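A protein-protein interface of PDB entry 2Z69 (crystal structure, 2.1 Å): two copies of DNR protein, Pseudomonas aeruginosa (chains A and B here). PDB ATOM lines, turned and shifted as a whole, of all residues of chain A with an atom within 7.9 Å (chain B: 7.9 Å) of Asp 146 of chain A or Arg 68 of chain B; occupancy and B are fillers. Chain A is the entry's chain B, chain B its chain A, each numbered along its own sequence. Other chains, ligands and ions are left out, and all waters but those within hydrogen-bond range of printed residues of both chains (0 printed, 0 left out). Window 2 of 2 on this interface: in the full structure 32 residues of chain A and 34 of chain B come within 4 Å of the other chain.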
ATOM      1  N   HIS A 142      -1.497  12.908  21.995  1.00  0.00           N
ATOM      2  CA  HIS A 142      -0.719  11.670  22.008  1.00  0.00           C
ATOM      3  C   HIS A 142      -0.069  11.521  20.641  1.00  0.00           C
ATOM      4  O   HIS A 142       0.867  10.738  20.468  1.00  0.00           O
ATOM      5  CB  HIS A 142      -1.593  10.465  22.329  1.00  0.00           C
ATOM      6  N   GLN A 143      -0.581  12.282  19.671  1.00  0.00           N
ATOM      7  CA  GLN A 143       0.165  12.569  18.448  1.00  0.00           C
ATOM      8  C   GLN A 143       1.318  13.484  18.843  1.00  0.00           C
ATOM      9  O   GLN A 143       2.148  13.857  18.012  1.00  0.00           O
ATOM     10  CB  GLN A 143      -0.724  13.235  17.406  1.00  0.00           C
ATOM     11  N   ARG A 144       1.340  13.840  20.127  1.00  0.00           N
ATOM     12  CA  ARG A 144       2.458  14.537  20.750  1.00  0.00           C
ATOM     13  C   ARG A 144       3.325  13.572  21.592  1.00  0.00           C
ATOM     14  O   ARG A 144       3.801  13.926  22.675  1.00  0.00           O
ATOM     15  CB  ARG A 144       1.946  15.715  21.585  1.00  0.00           C
ATOM     16  N   ILE A 145       3.535  12.361  21.066  1.00  0.00           N
ATOM     17  CA  ILE A 145       4.336  11.330  21.742  1.00  0.00           C
ATOM     18  C   ILE A 145       5.682  11.036  21.052  1.00  0.00           C
ATOM     19  O   ILE A 145       6.169   9.898  21.060  1.00  0.00           O
ATOM     20  CB  ILE A 145       3.522  10.048  21.916  1.00  0.00           C
ATOM     21  N   ASP A 146       6.267  12.067  20.449  1.00  0.00           N
ATOM     22  CA  ASP A 146       7.643  12.010  19.963  1.00  0.00           C
ATOM     23  C   ASP A 146       8.494  12.857  20.896  1.00  0.00           C
ATOM     24  O   ASP A 146       9.563  12.433  21.344  1.00  0.00           O
ATOM     25  CB  ASP A 146       7.738  12.526  18.521  1.00  0.00           C
ATOM     26  N   GLU A 147       7.989  14.056  21.186  1.00  0.00           N
ATOM     27  CA  GLU A 147       8.574  14.947  22.171  1.00  0.00           C
ATOM     28  C   GLU A 147       7.696  14.965  23.418  1.00  0.00           C
ATOM     29  O   GLU A 147       7.191  16.019  23.825  1.00  0.00           O
ATOM     30  CB  GLU A 147       8.735  16.355  21.592  1.00  0.00           C
ATOM     31  N   ILE A 148       7.501  13.780  24.004  1.00  0.00           N
ATOM     32  CA  ILE A 148       6.791  13.626  25.278  1.00  0.00           C
ATOM     33  C   ILE A 148       7.678  14.142  26.417  1.00  0.00           C
ATOM     34  O   ILE A 148       8.729  13.566  26.700  1.00  0.00           O
ATOM     35  CB  ILE A 148       6.395  12.160  25.500  1.00  0.00           C
ATOM     36  N   GLU A 149       7.259  15.240  27.045  1.00  0.00           N
ATOM     37  CA  GLU A 149       8.096  15.962  28.018  1.00  0.00           C
ATOM     38  C   GLU A 149       7.854  15.559  29.481  1.00  0.00           C
ATOM     39  O   GLU A 149       8.718  15.788  30.349  1.00  0.00           O
ATOM     40  CB  GLU A 149       7.910  17.471  27.848  1.00  0.00           C
ATOM     41  N   THR A 150       6.675  14.980  29.745  1.00  0.00           N
ATOM     42  CA  THR A 150       6.248  14.620  31.102  1.00  0.00           C
ATOM     43  C   THR A 150       5.265  13.457  31.102  1.00  0.00           C
ATOM     44  O   THR A 150       4.523  13.264  30.140  1.00  0.00           O
ATOM     45  CB  THR A 150       5.534  15.789  31.820  1.00  0.00           C
ATOM     46  OG1 THR A 150       6.144  17.038  31.472  1.00  0.00           O
ATOM     47  CG2 THR A 150       5.613  15.603  33.313  1.00  0.00           C
ATOM     48  N   ARG B  48      10.193   0.858  34.703  1.00  0.00           N
ATOM     49  CA  ARG B  48      11.111   1.170  33.633  1.00  0.00           C
ATOM     50  C   ARG B  48      10.460   1.462  32.291  1.00  0.00           C
ATOM     51  O   ARG B  48       9.412   0.906  31.970  1.00  0.00           O
ATOM     52  CB  ARG B  48      12.191   0.091  33.514  1.00  0.00           C
ATOM     53  CG  ARG B  48      13.507   0.550  34.054  1.00  0.00           C
ATOM     54  CD  ARG B  48      14.619   0.137  33.060  1.00  0.00           C
ATOM     55  NE  ARG B  48      15.945   0.716  33.315  1.00  0.00           N
ATOM     56  CZ  ARG B  48      16.450   1.789  32.696  1.00  0.00           C
ATOM     57  NH1 ARG B  48      15.738   2.456  31.792  1.00  0.00           N
ATOM     58  NH2 ARG B  48      17.673   2.208  32.999  1.00  0.00           N
ATOM     59  N   GLN B  49      11.122   2.342  31.524  1.00  0.00           N
ATOM     60  CA  GLN B  49      10.761   2.704  30.162  1.00  0.00           C
ATOM     61  C   GLN B  49      10.446   1.449  29.359  1.00  0.00           C
ATOM     62  O   GLN B  49      11.280   0.567  29.237  1.00  0.00           O
ATOM     63  CB  GLN B  49      11.953   3.441  29.527  1.00  0.00           C
ATOM     64  CG  GLN B  49      11.589   4.636  28.618  1.00  0.00           C
ATOM     65  CD  GLN B  49      11.624   4.102  27.053  1.00  0.00           C
ATOM     66  OE1 GLN B  49      11.267   2.934  26.680  1.00  0.00           O
ATOM     67  NE2 GLN B  49      12.029   5.151  26.221  1.00  0.00           N
ATOM     68  N   LYS B  65      13.691  10.437  39.979  1.00  0.00           N
ATOM     69  CA  LYS B  65      14.190  11.087  38.736  1.00  0.00           C
ATOM     70  C   LYS B  65      13.579  10.350  37.596  1.00  0.00           C
ATOM     71  O   LYS B  65      13.666   9.113  37.642  1.00  0.00           O
ATOM     72  CB  LYS B  65      15.747  11.128  38.610  1.00  0.00           C
ATOM     73  CG  LYS B  65      16.493   9.790  38.209  1.00  0.00           C
ATOM     74  CD  LYS B  65      17.968  10.060  37.723  1.00  0.00           C
ATOM     75  CE  LYS B  65      18.894   8.814  37.786  1.00  0.00           C
ATOM     76  NZ  LYS B  65      20.416   9.086  37.712  1.00  0.00           N
ATOM     77  N   ILE B  66      12.970  11.178  36.589  1.00  0.00           N
ATOM     78  CA  ILE B  66      12.247  10.592  35.460  1.00  0.00           C
ATOM     79  C   ILE B  66      12.854  11.106  34.190  1.00  0.00           C
ATOM     80  O   ILE B  66      12.978  12.315  34.014  1.00  0.00           O
ATOM     81  CB  ILE B  66      10.723  10.928  35.464  1.00  0.00           C
ATOM     82  CG1 ILE B  66      10.103  10.572  36.826  1.00  0.00           C
ATOM     83  CG2 ILE B  66      10.025  10.200  34.305  1.00  0.00           C
ATOM     84  CD1 ILE B  66       8.643  11.081  37.046  1.00  0.00           C
ATOM     85  N   TYR B  67      13.208  10.165  33.307  1.00  0.00           N
ATOM     86  CA  TYR B  67      14.013  10.445  32.143  1.00  0.00           C
ATOM     87  C   TYR B  67      13.783   9.377  31.073  1.00  0.00           C
ATOM     88  O   TYR B  67      13.430   8.215  31.395  1.00  0.00           O
ATOM     89  CB  TYR B  67      15.500  10.472  32.543  1.00  0.00           C
ATOM     90  CG  TYR B  67      15.968   9.199  33.218  1.00  0.00           C
ATOM     91  CD1 TYR B  67      15.867   9.039  34.612  1.00  0.00           C
ATOM     92  CD2 TYR B  67      16.507   8.149  32.468  1.00  0.00           C
ATOM     93  CE1 TYR B  67      16.310   7.862  35.236  1.00  0.00           C
ATOM     94  CE2 TYR B  67      16.944   6.974  33.077  1.00  0.00           C
ATOM     95  CZ  TYR B  67      16.844   6.835  34.459  1.00  0.00           C
ATOM     96  OH  TYR B  67      17.283   5.673  35.051  1.00  0.00           O
ATOM     97  N   ARG B  68      13.998   9.789  29.816  1.00  0.00           N
ATOM     98  CA  ARG B  68      13.856   8.938  28.625  1.00  0.00           C
ATOM     99  C   ARG B  68      15.216   8.508  28.105  1.00  0.00           C
ATOM    100  O   ARG B  68      16.245   9.027  28.548  1.00  0.00           O
ATOM    101  CB  ARG B  68      13.110   9.686  27.508  1.00  0.00           C
ATOM    102  CG  ARG B  68      11.652   9.981  27.804  1.00  0.00           C
ATOM    103  CD  ARG B  68      10.978  10.700  26.638  1.00  0.00           C
ATOM    104  NE  ARG B  68      10.422   9.772  25.643  1.00  0.00           N
ATOM    105  CZ  ARG B  68       9.892  10.144  24.476  1.00  0.00           C
ATOM    106  NH1 ARG B  68       9.837  11.434  24.132  1.00  0.00           N
ATOM    107  NH2 ARG B  68       9.413   9.222  23.644  1.00  0.00           N
ATOM    108  N   LEU B  69      15.203   7.570  27.151  1.00  0.00           N
ATOM    109  CA  LEU B  69      16.418   7.037  26.511  1.00  0.00           C
ATOM    110  C   LEU B  69      16.648   7.662  25.124  1.00  0.00           C
ATOM    111  O   LEU B  69      15.714   8.315  24.579  1.00  0.00           O
ATOM    112  CB  LEU B  69      16.332   5.520  26.409  1.00  0.00           C
ATOM    113  N   THR B  70      17.879   7.453  24.558  1.00  0.00           N
ATOM    114  CA  THR B  70      18.285   8.171  23.325  1.00  0.00           C
ATOM    115  C   THR B  70      18.452   7.263  22.073  1.00  0.00           C
ATOM    116  O   THR B  70      18.663   6.046  22.222  1.00  0.00           O
ATOM    117  CB  THR B  70      19.603   8.985  23.547  1.00  0.00           C
ATOM    118  OG1 THR B  70      20.749   8.077  23.670  1.00  0.00           O
ATOM    119  CG2 THR B  70      19.474   9.868  24.807  1.00  0.00           C
ATOM    120  N   ILE B  77      15.566  12.830  30.528  1.00  0.00           N
ATOM    121  CA  ILE B  77      15.880  14.271  30.806  1.00  0.00           C
ATOM    122  C   ILE B  77      14.571  15.013  31.122  1.00  0.00           C
ATOM    123  O   ILE B  77      14.298  16.089  30.562  1.00  0.00           O
ATOM    124  CB  ILE B  77      16.597  14.937  29.551  1.00  0.00           C
ATOM    125  N   LEU B  78      13.749  14.456  32.019  1.00  0.00           N
ATOM    126  CA  LEU B  78      12.346  14.898  32.071  1.00  0.00           C
ATOM    127  C   LEU B  78      11.882  15.763  33.263  1.00  0.00           C
ATOM    128  O   LEU B  78      11.456  16.918  33.068  1.00  0.00           O
ATOM    129  CB  LEU B  78      11.390  13.731  31.767  1.00  0.00           C
ATOM    130  CG  LEU B  78      11.476  13.080  30.374  1.00  0.00           C
ATOM    131  CD1 LEU B  78      10.331  12.099  30.194  1.00  0.00           C
ATOM    132  CD2 LEU B  78      11.450  14.130  29.254  1.00  0.00           C
ATOM    133  N   GLU B  79      11.974  15.216  34.477  1.00  0.00           N
ATOM    134  CA  GLU B  79      11.552  15.903  35.705  1.00  0.00           C
ATOM    135  C   GLU B  79      12.110  15.076  36.901  1.00  0.00           C
ATOM    136  O   GLU B  79      12.670  13.857  36.853  1.00  0.00           O
ATOM    137  CB  GLU B  79       9.967  15.972  35.800  1.00  0.00           C
ATOM    138  CG  GLU B  79       9.434  16.445  37.197  1.00  0.00           C
ATOM    139  CD  GLU B  79       7.898  16.447  37.319  1.00  0.00           C
ATOM    140  OE1 GLU B  79       7.191  16.809  36.330  1.00  0.00           O
ATOM    141  OE2 GLU B  79       7.389  16.094  38.425  1.00  0.00           O
ATOM    142  N   VAL B 100       6.303   4.982  29.017  1.00  0.00           N
ATOM    143  CA  VAL B 100       7.071   5.686  27.990  1.00  0.00           C
ATOM    144  C   VAL B 100       8.392   6.279  28.530  1.00  0.00           C
ATOM    145  O   VAL B 100       9.108   6.961  27.795  1.00  0.00           O
ATOM    146  CB  VAL B 100       6.175   6.781  27.315  1.00  0.00           C
ATOM    147  N   ALA B 101       8.700   6.006  29.811  1.00  0.00           N
ATOM    148  CA  ALA B 101       9.920   6.511  30.494  1.00  0.00           C
ATOM    149  C   ALA B 101      10.261   5.696  31.761  1.00  0.00           C
ATOM    150  O   ALA B 101       9.489   4.831  32.156  1.00  0.00           O
ATOM    151  CB  ALA B 101       9.774   7.989  30.844  1.00  0.00           C
ATOM    152  N   THR B 102      11.400   6.003  32.391  1.00  0.00           N
ATOM    153  CA  THR B 102      11.928   5.279  33.568  1.00  0.00           C
ATOM    154  C   THR B 102      11.953   6.185  34.790  1.00  0.00           C
ATOM    155  O   THR B 102      12.407   7.334  34.730  1.00  0.00           O
ATOM    156  CB  THR B 102      13.354   4.741  33.313  1.00  0.00           C
ATOM    157  OG1 THR B 102      13.307   3.724  32.311  1.00  0.00           O
ATOM    158  CG2 THR B 102      13.999   4.144  34.597  1.00  0.00           C
ATOM    159  N   ALA B 103      11.415   5.672  35.895  1.00  0.00           N
ATOM    160  CA  ALA B 103      11.453   6.371  37.161  1.00  0.00           C
ATOM    161  C   ALA B 103      12.318   5.516  38.087  1.00  0.00           C
ATOM    162  O   ALA B 103      12.079   4.298  38.221  1.00  0.00           O
ATOM    163  CB  ALA B 103      10.046   6.542  37.729  1.00  0.00           C
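Of the 9 printed residues of chain A, 4 touch a printed residue of chain B. Printed residues of chain A that touch a printed residue of chain B: Asp 146, Ile 148, Glu 149 and Thr 150. Hydrophobic or aromatic side chains of chain A that line the printed part of chain B: Ile 148. Along chain A the printed residues that touch a printed residue of chain B span positions 146 to 150. Printed residues of chain B that touch a printed residue of chain A: Arg 68, Leu 78 and Glu 79. Hydrophobic or aromatic side chains of chain B that line the printed part of chain A: Leu 78. Along chain B the printed residues that touch a printed residue of chain A span positions 68 to 79. Among the printed residues, 5 pairs touch across the chains.
No residue of chain B comes within 4 Å of Ile 145 of chain A. Asp 146 of chain A touches just one residue of chain B: Arg 68. Of the printed residues of chain B, Ile 148 of chain A touches Arg 68 (3.3 Å) and Leu 78 (3.8 Å). Of the printed residues of chain B, Thr 150 of chain A touches Glu 79. No residue of chain A comes within 4 Å of Leu 69 of chain B. Ile 77 of chain B touches none of the printed residues of chain A. Printed residues of chain A within 4 Å of Leu 78 of chain B: Ile 148 and Glu 149. The nearest printed residue of chain A that does not touch Arg 68 of chain B is Glu 147 of chain A (4.2 Å). The nearest printed residue of chain B that does not touch Ile 148 of chain A is Val 100 of chain B (5.7 Å).
Among the printed residues, merely in contact across the chains: Glu 149 of chain A with Leu 78 of chain B (3.4 Å), Thr 150 of chain A with Glu 79 of chain B (3.6 Å) and Ile 148 of chain A with Leu 78 of chain B (3.8 Å).
The guanidinium group (NH1) of Arg 68 of chain B sits at hydrogen-bond distance from the backbone carbonyl oxygen (O) of Asp 146 of chain A, 3.0 Å away. The backbone NH (N) of Ile 148 of chain A lies close to the guanidinium group (NH1) of Arg 68 of chain B (3.3 Å).
No position is printed for both chains.
N of Ile 66 of chain B lies within hydrogen-bond range of O of Glu 79 of chain B, 2.7 Å away. The backbone carbonyl oxygen (O) of Ile 66 of chain B lies within hydrogen-bond range of the backbone NH (N) of Leu 78 of chain B.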
